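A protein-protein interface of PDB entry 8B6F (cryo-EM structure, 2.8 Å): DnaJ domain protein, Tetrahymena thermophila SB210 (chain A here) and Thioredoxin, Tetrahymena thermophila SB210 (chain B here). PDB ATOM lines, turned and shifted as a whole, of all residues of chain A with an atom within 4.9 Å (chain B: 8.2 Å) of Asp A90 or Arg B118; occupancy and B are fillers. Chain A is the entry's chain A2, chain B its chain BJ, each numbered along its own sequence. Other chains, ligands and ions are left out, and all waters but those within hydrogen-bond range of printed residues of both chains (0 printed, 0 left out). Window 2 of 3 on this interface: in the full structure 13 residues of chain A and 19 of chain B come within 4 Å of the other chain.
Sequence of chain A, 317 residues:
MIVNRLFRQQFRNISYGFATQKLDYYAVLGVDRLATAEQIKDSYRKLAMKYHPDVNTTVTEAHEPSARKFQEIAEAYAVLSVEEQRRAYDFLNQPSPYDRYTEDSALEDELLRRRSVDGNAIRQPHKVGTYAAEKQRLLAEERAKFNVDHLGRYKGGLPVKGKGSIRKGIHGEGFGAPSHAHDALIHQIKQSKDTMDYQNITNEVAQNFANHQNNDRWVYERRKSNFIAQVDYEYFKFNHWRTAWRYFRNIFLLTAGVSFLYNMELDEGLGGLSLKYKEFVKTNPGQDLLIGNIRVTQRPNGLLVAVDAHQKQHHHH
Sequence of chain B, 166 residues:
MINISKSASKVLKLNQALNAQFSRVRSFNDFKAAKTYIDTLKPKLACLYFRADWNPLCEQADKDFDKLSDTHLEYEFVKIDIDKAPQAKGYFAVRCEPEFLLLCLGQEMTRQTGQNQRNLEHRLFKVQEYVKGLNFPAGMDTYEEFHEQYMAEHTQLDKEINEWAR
Asp A90 touches one residue of chain B.
Of chain A, only Glu A83 (3.4 Å), Arg A87 (3.9 Å), Asp A90 (3.2 Å) and Phe A91 (3.5 Å) come within 4 Å of Arg B118.
Of the printed residues of chain A, Glu B121 touches Arg A87 (2.9 Å) and Phe A91 (3.7 Å).
Of the printed residues of chain B, Phe A91 touches Arg B118 (3.5 Å), Glu B121 (3.7 Å), His B122 (3.5 Å) and Phe B125 (3.4 Å).
Of the printed residues of chain B, Glu A83 touches Arg B118.
Arg A86 touches none of the printed residues of chain B.
The nearest residue of chain B that does not touch Asp A90 is His B122 (5.8 Å).
OE2 of Glu A83 lies within salt-bridge range of NH1 of Arg B118 (3.4 Å).
The guanidinium group of Arg A87 is in salt-bridge range of the side-chain carboxylate of Glu B121, 2.9 Å away.
The side-chain carboxylate (OD1) of Asp A90 is in salt-bridge range of the guanidinium group (NH2) of Arg B118 (3.5 Å).
Of the 14 printed residues of chain A, 4 touch a printed residue of chain B.
Along chain A the printed residues that touch a printed residue of chain B span positions 83 to 91.
Among the printed residues, 9 pairs touch across the chains.
Among the printed residues, merely in contact across the chains: Phe A91 with Phe B125 (3.4 Å), Phe A91 with His B122 (3.5 Å), Phe A91 with Arg B118 (3.5 Å), Arg A87 with Gln B117 (3.5 Å), Phe A91 with Glu B121 (3.7 Å) and Arg A87 with Arg B118 (3.9 Å).
The guanidinium group (NE) of Arg A33 lies within salt-bridge range of the side-chain carboxylate (OD2) of Asp A90 (2.5 Å).
OD1 of Asp A90 is in hydrogen-bond range of OH of Tyr A26, 2.7 Å away.
The guanidinium group (NH2) of Arg A87 lies within salt-bridge range of the side-chain carboxylate (OE2) of Glu A83.
OD1 of Asp A90 lies close to O of Arg A86, at 2.6 Å.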
ATOM      1  N   TYR A  26      23.199  10.261  -6.719  1.00  0.00           N
ATOM      2  CA  TYR A  26      22.327  11.078  -7.554  1.00  0.00           C
ATOM      3  C   TYR A  26      22.910  11.258  -8.950  1.00  0.00           C
ATOM      4  O   TYR A  26      22.183  11.196  -9.948  1.00  0.00           O
ATOM      5  CB  TYR A  26      22.088  12.434  -6.891  1.00  0.00           C
ATOM      6  CG  TYR A  26      21.205  12.352  -5.669  1.00  0.00           C
ATOM      7  CD1 TYR A  26      19.824  12.382  -5.787  1.00  0.00           C
ATOM      8  CD2 TYR A  26      21.752  12.237  -4.401  1.00  0.00           C
ATOM      9  CE1 TYR A  26      19.010  12.304  -4.678  1.00  0.00           C
ATOM     10  CE2 TYR A  26      20.946  12.159  -3.284  1.00  0.00           C
ATOM     11  CZ  TYR A  26      19.577  12.190  -3.430  1.00  0.00           C
ATOM     12  OH  TYR A  26      18.769  12.113  -2.321  1.00  0.00           O
ATOM     13  N   ARG A  33      18.642  16.249  -6.751  1.00  0.00           N
ATOM     14  CA  ARG A  33      18.804  16.029  -5.320  1.00  0.00           C
ATOM     15  C   ARG A  33      17.453  15.954  -4.621  1.00  0.00           C
ATOM     16  O   ARG A  33      17.240  15.099  -3.755  1.00  0.00           O
ATOM     17  CB  ARG A  33      19.672  17.135  -4.720  1.00  0.00           C
ATOM     18  CG  ARG A  33      19.946  16.990  -3.234  1.00  0.00           C
ATOM     19  CD  ARG A  33      20.461  15.604  -2.893  1.00  0.00           C
ATOM     20  NE  ARG A  33      21.209  15.585  -1.642  1.00  0.00           N
ATOM     21  CZ  ARG A  33      22.529  15.686  -1.549  1.00  0.00           C
ATOM     22  NH1 ARG A  33      23.294  15.813  -2.621  1.00  0.00           N
ATOM     23  NH2 ARG A  33      23.098  15.658  -0.348  1.00  0.00           N
ATOM     24  N   LEU A  80      19.344   4.891  -2.091  1.00  0.00           N
ATOM     25  CA  LEU A  80      18.403   5.994  -2.233  1.00  0.00           C
ATOM     26  C   LEU A  80      16.947   5.569  -2.119  1.00  0.00           C
ATOM     27  O   LEU A  80      16.121   6.353  -1.641  1.00  0.00           O
ATOM     28  CB  LEU A  80      18.622   6.701  -3.572  1.00  0.00           C
ATOM     29  CG  LEU A  80      19.989   7.369  -3.754  1.00  0.00           C
ATOM     30  CD1 LEU A  80      20.122   7.867  -5.163  1.00  0.00           C
ATOM     31  CD2 LEU A  80      20.200   8.511  -2.777  1.00  0.00           C
ATOM     32  N   GLU A  83      13.861   5.277   2.363  1.00  0.00           N
ATOM     33  CA  GLU A  83      13.728   6.667   2.784  1.00  0.00           C
ATOM     34  C   GLU A  83      14.753   7.024   3.856  1.00  0.00           C
ATOM     35  O   GLU A  83      15.447   8.041   3.753  1.00  0.00           O
ATOM     36  CB  GLU A  83      12.308   6.921   3.290  1.00  0.00           C
ATOM     37  CG  GLU A  83      12.090   8.303   3.895  1.00  0.00           C
ATOM     38  CD  GLU A  83      12.440   9.428   2.941  1.00  0.00           C
ATOM     39  OE1 GLU A  83      12.533   9.174   1.722  1.00  0.00           O
ATOM     40  OE2 GLU A  83      12.621  10.570   3.411  1.00  0.00           O
ATOM     41  N   ARG A  86      18.343   7.003   2.451  1.00  0.00           N
ATOM     42  CA  ARG A  86      18.535   8.172   1.601  1.00  0.00           C
ATOM     43  C   ARG A  86      18.681   9.433   2.440  1.00  0.00           C
ATOM     44  O   ARG A  86      19.518  10.295   2.144  1.00  0.00           O
ATOM     45  CB  ARG A  86      17.364   8.317   0.630  1.00  0.00           C
ATOM     46  CG  ARG A  86      17.497   9.493  -0.324  1.00  0.00           C
ATOM     47  CD  ARG A  86      16.203   9.759  -1.066  1.00  0.00           C
ATOM     48  NE  ARG A  86      16.304  10.941  -1.911  1.00  0.00           N
ATOM     49  CZ  ARG A  86      15.284  11.487  -2.559  1.00  0.00           C
ATOM     50  NH1 ARG A  86      14.064  10.984  -2.477  1.00  0.00           N
ATOM     51  NH2 ARG A  86      15.494  12.565  -3.308  1.00  0.00           N
ATOM     52  N   ARG A  87      17.875   9.557   3.491  1.00  0.00           N
ATOM     53  CA  ARG A  87      17.976  10.712   4.373  1.00  0.00           C
ATOM     54  C   ARG A  87      19.348  10.776   5.031  1.00  0.00           C
ATOM     55  O   ARG A  87      19.963  11.846   5.099  1.00  0.00           O
ATOM     56  CB  ARG A  87      16.867  10.644   5.421  1.00  0.00           C
ATOM     57  CG  ARG A  87      16.810  11.823   6.363  1.00  0.00           C
ATOM     58  CD  ARG A  87      15.651  11.671   7.331  1.00  0.00           C
ATOM     59  NE  ARG A  87      14.376  11.563   6.634  1.00  0.00           N
ATOM     60  CZ  ARG A  87      13.220  11.286   7.219  1.00  0.00           C
ATOM     61  NH1 ARG A  87      13.138  11.072   8.522  1.00  0.00           N
ATOM     62  NH2 ARG A  87      12.118  11.215   6.479  1.00  0.00           N
ATOM     63  N   ALA A  88      19.843   9.641   5.521  1.00  0.00           N
ATOM     64  CA  ALA A  88      21.172   9.613   6.124  1.00  0.00           C
ATOM     65  C   ALA A  88      22.243   9.995   5.110  1.00  0.00           C
ATOM     66  O   ALA A  88      23.161  10.762   5.422  1.00  0.00           O
ATOM     67  CB  ALA A  88      21.453   8.230   6.707  1.00  0.00           C
ATOM     68  N   TYR A  89      22.145   9.465   3.889  1.00  0.00           N
ATOM     69  CA  TYR A  89      23.127   9.791   2.859  1.00  0.00           C
ATOM     70  C   TYR A  89      23.100  11.276   2.519  1.00  0.00           C
ATOM     71  O   TYR A  89      24.153  11.903   2.364  1.00  0.00           O
ATOM     72  CB  TYR A  89      22.872   8.952   1.606  1.00  0.00           C
ATOM     73  CG  TYR A  89      23.595   9.462   0.381  1.00  0.00           C
ATOM     74  CD1 TYR A  89      24.913   9.104   0.132  1.00  0.00           C
ATOM     75  CD2 TYR A  89      22.961  10.300  -0.525  1.00  0.00           C
ATOM     76  CE1 TYR A  89      25.580   9.570  -0.987  1.00  0.00           C
ATOM     77  CE2 TYR A  89      23.618  10.769  -1.645  1.00  0.00           C
ATOM     78  CZ  TYR A  89      24.926  10.400  -1.870  1.00  0.00           C
ATOM     79  OH  TYR A  89      25.580  10.868  -2.985  1.00  0.00           O
ATOM     80  N   ASP A  90      21.905  11.855   2.394  1.00  0.00           N
ATOM     81  CA  ASP A  90      21.805  13.277   2.086  1.00  0.00           C
ATOM     82  C   ASP A  90      22.408  14.128   3.196  1.00  0.00           C
ATOM     83  O   ASP A  90      23.119  15.101   2.923  1.00  0.00           O
ATOM     84  CB  ASP A  90      20.345  13.667   1.859  1.00  0.00           C
ATOM     85  CG  ASP A  90      19.844  13.272   0.486  1.00  0.00           C
ATOM     86  OD1 ASP A  90      19.629  12.066   0.252  1.00  0.00           O
ATOM     87  OD2 ASP A  90      19.666  14.169  -0.363  1.00  0.00           O
ATOM     88  N   PHE A  91      22.135  13.780   4.453  1.00  0.00           N
ATOM     89  CA  PHE A  91      22.711  14.534   5.561  1.00  0.00           C
ATOM     90  C   PHE A  91      24.230  14.425   5.570  1.00  0.00           C
ATOM     91  O   PHE A  91      24.929  15.416   5.803  1.00  0.00           O
ATOM     92  CB  PHE A  91      22.132  14.043   6.888  1.00  0.00           C
ATOM     93  CG  PHE A  91      20.651  14.281   7.037  1.00  0.00           C
ATOM     94  CD1 PHE A  91      19.943  15.010   6.094  1.00  0.00           C
ATOM     95  CD2 PHE A  91      19.971  13.783   8.135  1.00  0.00           C
ATOM     96  CE1 PHE A  91      18.590  15.226   6.239  1.00  0.00           C
ATOM     97  CE2 PHE A  91      18.617  13.996   8.283  1.00  0.00           C
ATOM     98  CZ  PHE A  91      17.926  14.717   7.334  1.00  0.00           C
ATOM     99  N   LEU A  92      24.760  13.228   5.312  1.00  0.00           N
ATOM    100  CA  LEU A  92      26.208  13.045   5.326  1.00  0.00           C
ATOM    101  C   LEU A  92      26.873  13.821   4.196  1.00  0.00           C
ATOM    102  O   LEU A  92      27.889  14.492   4.406  1.00  0.00           O
ATOM    103  CB  LEU A  92      26.547  11.557   5.238  1.00  0.00           C
ATOM    104  CG  LEU A  92      26.196  10.714   6.467  1.00  0.00           C
ATOM    105  CD1 LEU A  92      26.435   9.237   6.194  1.00  0.00           C
ATOM    106  CD2 LEU A  92      26.990  11.163   7.685  1.00  0.00           C
ATOM    107  N   ASN A  93      26.315  13.742   2.990  1.00  0.00           N
ATOM    108  CA  ASN A  93      26.871  14.416   1.821  1.00  0.00           C
ATOM    109  C   ASN A  93      26.058  15.680   1.563  1.00  0.00           C
ATOM    110  O   ASN A  93      24.933  15.609   1.060  1.00  0.00           O
ATOM    111  CB  ASN A  93      26.850  13.496   0.603  1.00  0.00           C
ATOM    112  CG  ASN A  93      27.603  12.205   0.839  1.00  0.00           C
ATOM    113  OD1 ASN A  93      28.787  12.098   0.523  1.00  0.00           O
ATOM    114  ND2 ASN A  93      26.919  11.216   1.401  1.00  0.00           N
ATOM    115  N   GLN A  94      26.630  16.829   1.897  1.00  0.00           N
ATOM    116  CA  GLN A  94      25.921  18.082   1.705  1.00  0.00           C
ATOM    117  C   GLN A  94      25.685  18.316   0.213  1.00  0.00           C
ATOM    118  O   GLN A  94      26.556  18.004  -0.607  1.00  0.00           O
ATOM    119  CB  GLN A  94      26.711  19.246   2.305  1.00  0.00           C
ATOM    120  CG  GLN A  94      25.986  20.584   2.233  1.00  0.00           C
ATOM    121  CD  GLN A  94      26.791  21.716   2.838  1.00  0.00           C
ATOM    122  OE1 GLN A  94      27.947  21.538   3.218  1.00  0.00           O
ATOM    123  NE2 GLN A  94      26.180  22.892   2.932  1.00  0.00           N
ATOM    124  N   PRO A  95      24.528  18.851  -0.178  1.00  0.00           N
ATOM    125  CA  PRO A  95      24.296  19.113  -1.603  1.00  0.00           C
ATOM    126  C   PRO A  95      25.338  20.068  -2.160  1.00  0.00           C
ATOM    127  O   PRO A  95      25.777  21.003  -1.487  1.00  0.00           O
ATOM    128  CB  PRO A  95      22.892  19.732  -1.631  1.00  0.00           C
ATOM    129  CG  PRO A  95      22.250  19.287  -0.370  1.00  0.00           C
ATOM    130  CD  PRO A  95      23.351  19.195   0.641  1.00  0.00           C
ATOM    131  N   ASP B  64       6.134  11.347  14.713  1.00  0.00           N
ATOM    132  CA  ASP B  64       7.476  11.643  14.224  1.00  0.00           C
ATOM    133  C   ASP B  64       8.457  11.785  15.378  1.00  0.00           C
ATOM    134  O   ASP B  64       9.577  11.267  15.323  1.00  0.00           O
ATOM    135  CB  ASP B  64       7.466  12.919  13.381  1.00  0.00           C
ATOM    136  CG  ASP B  64       6.651  12.773  12.112  1.00  0.00           C
ATOM    137  OD1 ASP B  64       6.084  11.684  11.890  1.00  0.00           O
ATOM    138  OD2 ASP B  64       6.581  13.746  11.335  1.00  0.00           O
ATOM    139  N   LEU B  68      11.771   9.355  16.017  1.00  0.00           N
ATOM    140  CA  LEU B  68      13.137   9.866  16.066  1.00  0.00           C
ATOM    141  C   LEU B  68      13.784   9.641  17.426  1.00  0.00           C
ATOM    142  O   LEU B  68      15.012   9.552  17.517  1.00  0.00           O
ATOM    143  CB  LEU B  68      13.153  11.353  15.717  1.00  0.00           C
ATOM    144  CG  LEU B  68      12.693  11.724  14.305  1.00  0.00           C
ATOM    145  CD1 LEU B  68      12.789  13.222  14.106  1.00  0.00           C
ATOM    146  CD2 LEU B  68      13.496  10.997  13.240  1.00  0.00           C
ATOM    147  N   GLN B 112      12.346  24.651  15.437  1.00  0.00           N
ATOM    148  CA  GLN B 112      11.558  24.317  14.263  1.00  0.00           C
ATOM    149  C   GLN B 112      10.081  24.486  14.575  1.00  0.00           C
ATOM    150  O   GLN B 112       9.613  24.094  15.647  1.00  0.00           O
ATOM    151  CB  GLN B 112      11.825  22.884  13.797  1.00  0.00           C
ATOM    152  CG  GLN B 112      10.857  22.399  12.725  1.00  0.00           C
ATOM    153  CD  GLN B 112      11.271  21.079  12.119  1.00  0.00           C
ATOM    154  OE1 GLN B 112      12.442  20.711  12.147  1.00  0.00           O
ATOM    155  NE2 GLN B 112      10.307  20.355  11.563  1.00  0.00           N
ATOM    156  N   GLN B 115       5.356  20.427  11.504  1.00  0.00           N
ATOM    157  CA  GLN B 115       5.655  19.002  11.487  1.00  0.00           C
ATOM    158  C   GLN B 115       6.376  18.669  10.187  1.00  0.00           C
ATOM    159  O   GLN B 115       5.803  18.790   9.100  1.00  0.00           O
ATOM    160  CB  GLN B 115       4.371  18.187  11.630  1.00  0.00           C
ATOM    161  CG  GLN B 115       4.562  16.685  11.485  1.00  0.00           C
ATOM    162  CD  GLN B 115       4.533  16.221  10.043  1.00  0.00           C
ATOM    163  OE1 GLN B 115       3.816  16.778   9.214  1.00  0.00           O
ATOM    164  NE2 GLN B 115       5.323  15.200   9.735  1.00  0.00           N
ATOM    165  N   ASN B 116       7.635  18.252  10.304  1.00  0.00           N
ATOM    166  CA  ASN B 116       8.370  17.714   9.163  1.00  0.00           C
ATOM    167  C   ASN B 116       9.484  16.840   9.720  1.00  0.00           C
ATOM    168  O   ASN B 116      10.459  17.360  10.271  1.00  0.00           O
ATOM    169  CB  ASN B 116       8.921  18.826   8.285  1.00  0.00           C
ATOM    170  CG  ASN B 116       9.301  18.336   6.904  1.00  0.00           C
ATOM    171  OD1 ASN B 116      10.427  17.903   6.673  1.00  0.00           O
ATOM    172  ND2 ASN B 116       8.353  18.392   5.977  1.00  0.00           N
ATOM    173  N   GLN B 117       9.336  15.522   9.581  1.00  0.00           N
ATOM    174  CA  GLN B 117      10.308  14.607  10.169  1.00  0.00           C
ATOM    175  C   GLN B 117      11.684  14.785   9.545  1.00  0.00           C
ATOM    176  O   GLN B 117      12.700  14.758  10.249  1.00  0.00           O
ATOM    177  CB  GLN B 117       9.826  13.166  10.013  1.00  0.00           C
ATOM    178  CG  GLN B 117      10.655  12.160  10.787  1.00  0.00           C
ATOM    179  CD  GLN B 117      10.075  10.766  10.720  1.00  0.00           C
ATOM    180  OE1 GLN B 117       9.029  10.545  10.116  1.00  0.00           O
ATOM    181  NE2 GLN B 117      10.755   9.813  11.347  1.00  0.00           N
ATOM    182  N   ARG B 118      11.743  14.962   8.225  1.00  0.00           N
ATOM    183  CA  ARG B 118      13.032  15.123   7.561  1.00  0.00           C
ATOM    184  C   ARG B 118      13.760  16.363   8.063  1.00  0.00           C
ATOM    185  O   ARG B 118      14.958  16.313   8.367  1.00  0.00           O
ATOM    186  CB  ARG B 118      12.833  15.194   6.049  1.00  0.00           C
ATOM    187  CG  ARG B 118      14.129  15.330   5.276  1.00  0.00           C
ATOM    188  CD  ARG B 118      14.116  14.474   4.026  1.00  0.00           C
ATOM    189  NE  ARG B 118      15.426  14.414   3.392  1.00  0.00           N
ATOM    190  CZ  ARG B 118      15.750  13.573   2.421  1.00  0.00           C
ATOM    191  NH1 ARG B 118      14.880  12.700   1.944  1.00  0.00           N
ATOM    192  NH2 ARG B 118      16.980  13.606   1.917  1.00  0.00           N
ATOM    193  N   ASN B 119      13.058  17.493   8.151  1.00  0.00           N
ATOM    194  CA  ASN B 119      13.700  18.718   8.613  1.00  0.00           C
ATOM    195  C   ASN B 119      14.107  18.612  10.077  1.00  0.00           C
ATOM    196  O   ASN B 119      15.174  19.099  10.466  1.00  0.00           O
ATOM    197  CB  ASN B 119      12.774  19.914   8.400  1.00  0.00           C
ATOM    198  CG  ASN B 119      12.536  20.209   6.934  1.00  0.00           C
ATOM    199  OD1 ASN B 119      11.397  20.318   6.487  1.00  0.00           O
ATOM    200  ND2 ASN B 119      13.617  20.344   6.174  1.00  0.00           N
ATOM    201  N   LEU B 120      13.270  17.988  10.906  1.00  0.00           N
ATOM    202  CA  LEU B 120      13.626  17.819  12.310  1.00  0.00           C
ATOM    203  C   LEU B 120      14.879  16.969  12.458  1.00  0.00           C
ATOM    204  O   LEU B 120      15.780  17.307  13.233  1.00  0.00           O
ATOM    205  CB  LEU B 120      12.456  17.199  13.074  1.00  0.00           C
ATOM    206  CG  LEU B 120      12.648  16.995  14.578  1.00  0.00           C
ATOM    207  CD1 LEU B 120      12.988  18.299  15.279  1.00  0.00           C
ATOM    208  CD2 LEU B 120      11.395  16.384  15.174  1.00  0.00           C
ATOM    209  N   GLU B 121      14.959  15.864  11.715  1.00  0.00           N
ATOM    210  CA  GLU B 121      16.140  15.012  11.783  1.00  0.00           C
ATOM    211  C   GLU B 121      17.369  15.735  11.249  1.00  0.00           C
ATOM    212  O   GLU B 121      18.473  15.573  11.783  1.00  0.00           O
ATOM    213  CB  GLU B 121      15.899  13.716  11.014  1.00  0.00           C
ATOM    214  CG  GLU B 121      16.945  12.651  11.292  1.00  0.00           C
ATOM    215  CD  GLU B 121      16.590  11.311  10.681  1.00  0.00           C
ATOM    216  OE1 GLU B 121      15.434  11.144  10.241  1.00  0.00           O
ATOM    217  OE2 GLU B 121      17.469  10.423  10.643  1.00  0.00           O
ATOM    218  N   HIS B 122      17.199  16.541  10.199  1.00  0.00           N
ATOM    219  CA  HIS B 122      18.320  17.311   9.673  1.00  0.00           C
ATOM    220  C   HIS B 122      18.832  18.304  10.707  1.00  0.00           C
ATOM    221  O   HIS B 122      20.045  18.478  10.864  1.00  0.00           O
ATOM    222  CB  HIS B 122      17.901  18.038   8.394  1.00  0.00           C
ATOM    223  CG  HIS B 122      19.052  18.493   7.551  1.00  0.00           C
ATOM    224  ND1 HIS B 122      20.367  18.237   7.881  1.00  0.00           N
ATOM    225  CD2 HIS B 122      19.084  19.182   6.386  1.00  0.00           C
ATOM    226  CE1 HIS B 122      21.158  18.752   6.957  1.00  0.00           C
ATOM    227  NE2 HIS B 122      20.405  19.330   6.038  1.00  0.00           N
ATOM    228  N   ARG B 123      17.922  18.970  11.422  1.00  0.00           N
ATOM    229  CA  ARG B 123      18.345  19.888  12.473  1.00  0.00           C
ATOM    230  C   ARG B 123      19.079  19.147  13.582  1.00  0.00           C
ATOM    231  O   ARG B 123      20.099  19.628  14.089  1.00  0.00           O
ATOM    232  CB  ARG B 123      17.137  20.635  13.036  1.00  0.00           C
ATOM    233  CG  ARG B 123      16.503  21.596  12.049  1.00  0.00           C
ATOM    234  CD  ARG B 123      15.297  22.293  12.649  1.00  0.00           C
ATOM    235  NE  ARG B 123      14.527  23.002  11.634  1.00  0.00           N
ATOM    236  CZ  ARG B 123      14.801  24.222  11.193  1.00  0.00           C
ATOM    237  NH1 ARG B 123      15.834  24.909  11.652  1.00  0.00           N
ATOM    238  NH2 ARG B 123      14.019  24.767  10.266  1.00  0.00           N
ATOM    239  N   LEU B 124      18.574  17.976  13.977  1.00  0.00           N
ATOM    240  CA  LEU B 124      19.267  17.186  14.989  1.00  0.00           C
ATOM    241  C   LEU B 124      20.672  16.831  14.524  1.00  0.00           C
ATOM    242  O   LEU B 124      21.635  16.928  15.293  1.00  0.00           O
ATOM    243  CB  LEU B 124      18.474  15.919  15.306  1.00  0.00           C
ATOM    244  CG  LEU B 124      17.140  16.115  16.028  1.00  0.00           C
ATOM    245  CD1 LEU B 124      16.360  14.817  16.055  1.00  0.00           C
ATOM    246  CD2 LEU B 124      17.355  16.628  17.438  1.00  0.00           C
ATOM    247  N   PHE B 125      20.805  16.405  13.267  1.00  0.00           N
ATOM    248  CA  PHE B 125      22.115  16.040  12.741  1.00  0.00           C
ATOM    249  C   PHE B 125      23.056  17.238  12.738  1.00  0.00           C
ATOM    250  O   PHE B 125      24.223  17.127  13.126  1.00  0.00           O
ATOM    251  CB  PHE B 125      21.959  15.467  11.332  1.00  0.00           C
ATOM    252  CG  PHE B 125      23.261  15.166  10.651  1.00  0.00           C
ATOM    253  CD1 PHE B 125      23.893  13.951  10.846  1.00  0.00           C
ATOM    254  CD2 PHE B 125      23.845  16.092   9.805  1.00  0.00           C
ATOM    255  CE1 PHE B 125      25.088  13.668  10.215  1.00  0.00           C
ATOM    256  CE2 PHE B 125      25.038  15.816   9.171  1.00  0.00           C
ATOM    257  CZ  PHE B 125      25.661  14.603   9.376  1.00  0.00           C
